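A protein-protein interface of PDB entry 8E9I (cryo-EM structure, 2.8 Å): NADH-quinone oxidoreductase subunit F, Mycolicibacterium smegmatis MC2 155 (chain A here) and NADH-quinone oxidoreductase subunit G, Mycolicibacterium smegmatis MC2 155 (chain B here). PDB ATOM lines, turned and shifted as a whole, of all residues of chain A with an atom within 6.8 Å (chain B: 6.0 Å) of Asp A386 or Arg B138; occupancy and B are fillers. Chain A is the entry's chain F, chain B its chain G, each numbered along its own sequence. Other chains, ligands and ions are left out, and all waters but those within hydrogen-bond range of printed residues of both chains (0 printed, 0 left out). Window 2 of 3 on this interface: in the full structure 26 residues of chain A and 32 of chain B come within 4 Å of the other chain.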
ATOM      1  N   TRP A 363     -18.860 -16.614  17.709  1.00  0.00           N
ATOM      2  CA  TRP A 363     -18.689 -15.364  18.437  1.00  0.00           C
ATOM      3  C   TRP A 363     -19.266 -14.188  17.662  1.00  0.00           C
ATOM      4  O   TRP A 363     -19.922 -13.318  18.238  1.00  0.00           O
ATOM      5  CB  TRP A 363     -17.210 -15.141  18.732  1.00  0.00           C
ATOM      6  CG  TRP A 363     -16.951 -14.049  19.697  1.00  0.00           C
ATOM      7  CD1 TRP A 363     -17.873 -13.333  20.395  1.00  0.00           C
ATOM      8  CD2 TRP A 363     -15.674 -13.541  20.078  1.00  0.00           C
ATOM      9  NE1 TRP A 363     -17.249 -12.406  21.190  1.00  0.00           N
ATOM     10  CE2 TRP A 363     -15.896 -12.518  21.015  1.00  0.00           C
ATOM     11  CE3 TRP A 363     -14.363 -13.857  19.724  1.00  0.00           C
ATOM     12  CZ2 TRP A 363     -14.858 -11.808  21.597  1.00  0.00           C
ATOM     13  CZ3 TRP A 363     -13.337 -13.152  20.300  1.00  0.00           C
ATOM     14  CH2 TRP A 363     -13.587 -12.139  21.227  1.00  0.00           C
ATOM     15  N   LEU A 364     -19.020 -14.135  16.355  1.00  0.00           N
ATOM     16  CA  LEU A 364     -19.523 -13.028  15.552  1.00  0.00           C
ATOM     17  C   LEU A 364     -21.039 -13.058  15.475  1.00  0.00           C
ATOM     18  O   LEU A 364     -21.692 -12.012  15.485  1.00  0.00           O
ATOM     19  CB  LEU A 364     -18.923 -13.076  14.153  1.00  0.00           C
ATOM     20  CG  LEU A 364     -17.424 -12.818  14.072  1.00  0.00           C
ATOM     21  CD1 LEU A 364     -16.865 -13.405  12.795  1.00  0.00           C
ATOM     22  CD2 LEU A 364     -17.141 -11.337  14.166  1.00  0.00           C
ATOM     23  N   ARG A 370     -26.246  -9.220  19.583  1.00  0.00           N
ATOM     24  CA  ARG A 370     -26.266  -8.088  20.504  1.00  0.00           C
ATOM     25  C   ARG A 370     -26.496  -6.780  19.756  1.00  0.00           C
ATOM     26  O   ARG A 370     -27.271  -5.927  20.201  1.00  0.00           O
ATOM     27  CB  ARG A 370     -24.964  -8.023  21.294  1.00  0.00           C
ATOM     28  CG  ARG A 370     -24.945  -8.876  22.537  1.00  0.00           C
ATOM     29  CD  ARG A 370     -23.705  -8.581  23.346  1.00  0.00           C
ATOM     30  NE  ARG A 370     -22.502  -8.729  22.540  1.00  0.00           N
ATOM     31  CZ  ARG A 370     -21.302  -8.304  22.900  1.00  0.00           C
ATOM     32  NH1 ARG A 370     -21.106  -7.678  24.049  1.00  0.00           N
ATOM     33  NH2 ARG A 370     -20.271  -8.507  22.086  1.00  0.00           N
ATOM     34  N   ILE A 381     -17.745  -3.019  17.433  1.00  0.00           N
ATOM     35  CA  ILE A 381     -17.359  -2.970  16.024  1.00  0.00           C
ATOM     36  C   ILE A 381     -15.886  -3.314  15.863  1.00  0.00           C
ATOM     37  O   ILE A 381     -15.500  -4.087  14.975  1.00  0.00           O
ATOM     38  CB  ILE A 381     -17.678  -1.588  15.430  1.00  0.00           C
ATOM     39  CG1 ILE A 381     -19.181  -1.325  15.485  1.00  0.00           C
ATOM     40  CG2 ILE A 381     -17.177  -1.507  14.002  1.00  0.00           C
ATOM     41  CD1 ILE A 381     -19.622  -0.605  16.721  1.00  0.00           C
ATOM     42  N   ASP A 382     -15.036  -2.734  16.708  1.00  0.00           N
ATOM     43  CA  ASP A 382     -13.622  -3.069  16.649  1.00  0.00           C
ATOM     44  C   ASP A 382     -13.410  -4.552  16.910  1.00  0.00           C
ATOM     45  O   ASP A 382     -12.567  -5.185  16.266  1.00  0.00           O
ATOM     46  CB  ASP A 382     -12.840  -2.225  17.653  1.00  0.00           C
ATOM     47  N   LYS A 383     -14.165  -5.124  17.851  1.00  0.00           N
ATOM     48  CA  LYS A 383     -14.074  -6.561  18.087  1.00  0.00           C
ATOM     49  C   LYS A 383     -14.502  -7.349  16.860  1.00  0.00           C
ATOM     50  O   LYS A 383     -13.894  -8.369  16.527  1.00  0.00           O
ATOM     51  CB  LYS A 383     -14.928  -6.960  19.284  1.00  0.00           C
ATOM     52  CG  LYS A 383     -14.274  -6.714  20.627  1.00  0.00           C
ATOM     53  CD  LYS A 383     -15.034  -7.404  21.752  1.00  0.00           C
ATOM     54  CE  LYS A 383     -16.450  -6.871  21.897  1.00  0.00           C
ATOM     55  NZ  LYS A 383     -17.200  -7.570  22.970  1.00  0.00           N
ATOM     56  N   LEU A 384     -15.566  -6.913  16.189  1.00  0.00           N
ATOM     57  CA  LEU A 384     -15.990  -7.607  14.982  1.00  0.00           C
ATOM     58  C   LEU A 384     -14.870  -7.617  13.958  1.00  0.00           C
ATOM     59  O   LEU A 384     -14.571  -8.656  13.360  1.00  0.00           O
ATOM     60  CB  LEU A 384     -17.235  -6.944  14.395  1.00  0.00           C
ATOM     61  CG  LEU A 384     -18.576  -7.213  15.080  1.00  0.00           C
ATOM     62  CD1 LEU A 384     -19.671  -6.438  14.387  1.00  0.00           C
ATOM     63  CD2 LEU A 384     -18.906  -8.688  15.088  1.00  0.00           C
ATOM     64  N   LEU A 385     -14.223  -6.472  13.761  1.00  0.00           N
ATOM     65  CA  LEU A 385     -13.137  -6.405  12.790  1.00  0.00           C
ATOM     66  C   LEU A 385     -11.963  -7.279  13.213  1.00  0.00           C
ATOM     67  O   LEU A 385     -11.375  -7.986  12.387  1.00  0.00           O
ATOM     68  CB  LEU A 385     -12.688  -4.958  12.591  1.00  0.00           C
ATOM     69  CG  LEU A 385     -13.547  -4.131  11.631  1.00  0.00           C
ATOM     70  CD1 LEU A 385     -13.023  -2.714  11.543  1.00  0.00           C
ATOM     71  CD2 LEU A 385     -13.596  -4.762  10.252  1.00  0.00           C
ATOM     72  N   ASP A 386     -11.601  -7.243  14.496  1.00  0.00           N
ATOM     73  CA  ASP A 386     -10.477  -8.047  14.962  1.00  0.00           C
ATOM     74  C   ASP A 386     -10.758  -9.535  14.796  1.00  0.00           C
ATOM     75  O   ASP A 386      -9.885 -10.296  14.362  1.00  0.00           O
ATOM     76  CB  ASP A 386     -10.172  -7.719  16.422  1.00  0.00           C
ATOM     77  N   ILE A 387     -11.970  -9.968  15.131  1.00  0.00           N
ATOM     78  CA  ILE A 387     -12.322 -11.375  14.985  1.00  0.00           C
ATOM     79  C   ILE A 387     -12.310 -11.770  13.516  1.00  0.00           C
ATOM     80  O   ILE A 387     -11.790 -12.829  13.146  1.00  0.00           O
ATOM     81  CB  ILE A 387     -13.691 -11.652  15.631  1.00  0.00           C
ATOM     82  CG1 ILE A 387     -13.643 -11.385  17.132  1.00  0.00           C
ATOM     83  CG2 ILE A 387     -14.112 -13.079  15.388  1.00  0.00           C
ATOM     84  CD1 ILE A 387     -14.992 -11.072  17.726  1.00  0.00           C
ATOM     85  N   SER A 388     -12.876 -10.923  12.654  1.00  0.00           N
ATOM     86  CA  SER A 388     -12.861 -11.223  11.229  1.00  0.00           C
ATOM     87  C   SER A 388     -11.435 -11.360  10.725  1.00  0.00           C
ATOM     88  O   SER A 388     -11.132 -12.252   9.927  1.00  0.00           O
ATOM     89  CB  SER A 388     -13.597 -10.133  10.456  1.00  0.00           C
ATOM     90  OG  SER A 388     -12.851  -8.930  10.462  1.00  0.00           O
ATOM     91  N   ASP A 389     -10.543 -10.483  11.182  1.00  0.00           N
ATOM     92  CA  ASP A 389      -9.140 -10.593  10.802  1.00  0.00           C
ATOM     93  C   ASP A 389      -8.559 -11.917  11.270  1.00  0.00           C
ATOM     94  O   ASP A 389      -7.817 -12.580  10.535  1.00  0.00           O
ATOM     95  CB  ASP A 389      -8.350  -9.423  11.384  1.00  0.00           C
ATOM     96  N   ASN A 390      -8.884 -12.319  12.500  1.00  0.00           N
ATOM     97  CA  ASN A 390      -8.394 -13.585  13.025  1.00  0.00           C
ATOM     98  C   ASN A 390      -8.958 -14.788  12.290  1.00  0.00           C
ATOM     99  O   ASN A 390      -8.366 -15.868  12.368  1.00  0.00           O
ATOM    100  CB  ASN A 390      -8.728 -13.712  14.505  1.00  0.00           C
ATOM    101  CG  ASN A 390      -7.897 -12.805  15.363  1.00  0.00           C
ATOM    102  OD1 ASN A 390      -6.869 -12.292  14.928  1.00  0.00           O
ATOM    103  ND2 ASN A 390      -8.332 -12.604  16.599  1.00  0.00           N
ATOM    104  N   ILE A 391     -10.086 -14.646  11.601  1.00  0.00           N
ATOM    105  CA  ILE A 391     -10.645 -15.751  10.831  1.00  0.00           C
ATOM    106  C   ILE A 391     -10.094 -15.711   9.415  1.00  0.00           C
ATOM    107  O   ILE A 391      -9.595 -16.718   8.903  1.00  0.00           O
ATOM    108  CB  ILE A 391     -12.182 -15.709  10.813  1.00  0.00           C
ATOM    109  CG1 ILE A 391     -12.730 -15.827  12.231  1.00  0.00           C
ATOM    110  CG2 ILE A 391     -12.727 -16.820   9.934  1.00  0.00           C
ATOM    111  CD1 ILE A 391     -14.226 -15.765  12.301  1.00  0.00           C
ATOM    112  N   GLU B 104      -7.339 -17.083  21.429  1.00  0.00           N
ATOM    113  CA  GLU B 104      -8.537 -16.446  21.963  1.00  0.00           C
ATOM    114  C   GLU B 104      -9.786 -17.189  21.522  1.00  0.00           C
ATOM    115  O   GLU B 104     -10.622 -17.568  22.348  1.00  0.00           O
ATOM    116  CB  GLU B 104      -8.606 -14.989  21.516  1.00  0.00           C
ATOM    117  CG  GLU B 104      -9.981 -14.365  21.663  1.00  0.00           C
ATOM    118  CD  GLU B 104      -9.993 -12.914  21.271  1.00  0.00           C
ATOM    119  OE1 GLU B 104      -9.445 -12.583  20.203  1.00  0.00           O
ATOM    120  OE2 GLU B 104     -10.560 -12.101  22.023  1.00  0.00           O
ATOM    121  N   ARG B 134      -3.766 -13.868  25.204  1.00  0.00           N
ATOM    122  CA  ARG B 134      -4.036 -12.539  25.710  1.00  0.00           C
ATOM    123  C   ARG B 134      -4.121 -12.571  27.230  1.00  0.00           C
ATOM    124  O   ARG B 134      -4.442 -13.603  27.821  1.00  0.00           O
ATOM    125  CB  ARG B 134      -5.337 -12.014  25.115  1.00  0.00           C
ATOM    126  CG  ARG B 134      -5.357 -12.042  23.598  1.00  0.00           C
ATOM    127  CD  ARG B 134      -6.661 -11.523  23.007  1.00  0.00           C
ATOM    128  NE  ARG B 134      -7.054 -10.229  23.549  1.00  0.00           N
ATOM    129  CZ  ARG B 134      -7.811 -10.063  24.620  1.00  0.00           C
ATOM    130  NH1 ARG B 134      -8.245 -11.094  25.326  1.00  0.00           N
ATOM    131  NH2 ARG B 134      -8.138  -8.833  24.998  1.00  0.00           N
ATOM    132  N   GLU B 136      -6.378 -11.283  29.249  1.00  0.00           N
ATOM    133  CA  GLU B 136      -7.717 -11.404  29.811  1.00  0.00           C
ATOM    134  C   GLU B 136      -8.729 -11.618  28.697  1.00  0.00           C
ATOM    135  O   GLU B 136      -8.429 -11.432  27.516  1.00  0.00           O
ATOM    136  CB  GLU B 136      -8.091 -10.164  30.628  1.00  0.00           C
ATOM    137  N   THR B 137      -9.939 -12.017  29.087  1.00  0.00           N
ATOM    138  CA  THR B 137     -10.992 -12.232  28.106  1.00  0.00           C
ATOM    139  C   THR B 137     -11.371 -10.943  27.397  1.00  0.00           C
ATOM    140  O   THR B 137     -11.362  -9.853  27.972  1.00  0.00           O
ATOM    141  CB  THR B 137     -12.258 -12.818  28.740  1.00  0.00           C
ATOM    142  OG1 THR B 137     -12.709 -11.983  29.816  1.00  0.00           O
ATOM    143  CG2 THR B 137     -12.063 -14.239  29.185  1.00  0.00           C
ATOM    144  N   ARG B 138     -11.703 -11.098  26.123  1.00  0.00           N
ATOM    145  CA  ARG B 138     -12.427 -10.111  25.353  1.00  0.00           C
ATOM    146  C   ARG B 138     -13.858 -10.550  25.086  1.00  0.00           C
ATOM    147  O   ARG B 138     -14.632  -9.774  24.516  1.00  0.00           O
ATOM    148  CB  ARG B 138     -11.706  -9.869  24.023  1.00  0.00           C
ATOM    149  CG  ARG B 138     -12.192  -8.694  23.221  1.00  0.00           C
ATOM    150  CD  ARG B 138     -11.070  -8.184  22.348  1.00  0.00           C
ATOM    151  NE  ARG B 138     -10.529  -9.246  21.509  1.00  0.00           N
ATOM    152  CZ  ARG B 138      -9.759  -9.046  20.450  1.00  0.00           C
ATOM    153  NH1 ARG B 138      -9.390  -7.832  20.081  1.00  0.00           N
ATOM    154  NH2 ARG B 138      -9.343 -10.093  19.744  1.00  0.00           N
ATOM    155  N   PHE B 139     -14.229 -11.758  25.500  1.00  0.00           N
ATOM    156  CA  PHE B 139     -15.497 -12.379  25.140  1.00  0.00           C
ATOM    157  C   PHE B 139     -16.511 -12.140  26.249  1.00  0.00           C
ATOM    158  O   PHE B 139     -16.475 -12.807  27.285  1.00  0.00           O
ATOM    159  CB  PHE B 139     -15.276 -13.871  24.907  1.00  0.00           C
ATOM    160  CG  PHE B 139     -16.525 -14.648  24.638  1.00  0.00           C
ATOM    161  CD1 PHE B 139     -17.049 -14.728  23.367  1.00  0.00           C
ATOM    162  CD2 PHE B 139     -17.158 -15.329  25.655  1.00  0.00           C
ATOM    163  CE1 PHE B 139     -18.188 -15.456  23.119  1.00  0.00           C
ATOM    164  CE2 PHE B 139     -18.297 -16.057  25.412  1.00  0.00           C
ATOM    165  CZ  PHE B 139     -18.813 -16.119  24.142  1.00  0.00           C
ATOM    166  N   GLU B 140     -17.422 -11.196  26.035  1.00  0.00           N
ATOM    167  CA  GLU B 140     -18.487 -10.917  26.987  1.00  0.00           C
ATOM    168  C   GLU B 140     -19.786 -11.633  26.648  1.00  0.00           C
ATOM    169  O   GLU B 140     -20.770 -11.473  27.372  1.00  0.00           O
ATOM    170  CB  GLU B 140     -18.741  -9.410  27.066  1.00  0.00           C
ATOM    171  N   ASP B 141     -19.813 -12.413  25.572  1.00  0.00           N
ATOM    172  CA  ASP B 141     -21.024 -13.108  25.155  1.00  0.00           C
ATOM    173  C   ASP B 141     -21.221 -14.394  25.950  1.00  0.00           C
ATOM    174  O   ASP B 141     -20.588 -14.591  26.990  1.00  0.00           O
ATOM    175  CB  ASP B 141     -20.971 -13.408  23.658  1.00  0.00           C
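Among the printed residues, pairs that only touch across the chains: Trp A363 with Glu B104 (3.1 Å), Trp A363 with Arg B138 (3.6 Å), Trp A363 with Phe B139 (3.2 Å), Lys A383 with Arg B138 (3.4 Å), Asp A386 with Arg B138 (3.7 Å) and Asn A390 with Glu B104 (3.8 Å).
The side-chain carboxylate of Glu B104 is in salt-bridge range of the guanidinium group of Arg B138, 2.5 Å away.
Printed residues of chain B within 4 Å of Trp A363: Glu B104, Arg B138 and Phe B139.
Of the printed residues of chain B, Asp A386 touches Arg B138.
Of the printed residues of chain A, Glu B104 touches Trp A363 and Asn A390.
Of chain A, only Trp A363, Lys A383 and Asp A386 come within 4 Å of Arg B138.
Printed residues of chain A within 4 Å of Phe B139: Trp A363.
Of the 8 printed residues of chain B, 3 touch a printed residue of chain A.
Hydrophobic or aromatic side chains of chain B within 4 Å of the printed part of chain A: Phe B139.
Printed residues of chain A that touch a printed residue of chain B: Trp A363, Lys A383, Asp A386 and Asn A390.
Hydrophobic or aromatic side chains of chain A within 4 Å of the printed part of chain B: Trp A363.
Among the printed residues, 6 pairs touch across the chains.
Among the printed residues, no Asp or Glu carboxylate lies within 4 Å of a Lys or Arg side-chain nitrogen of the other chain.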
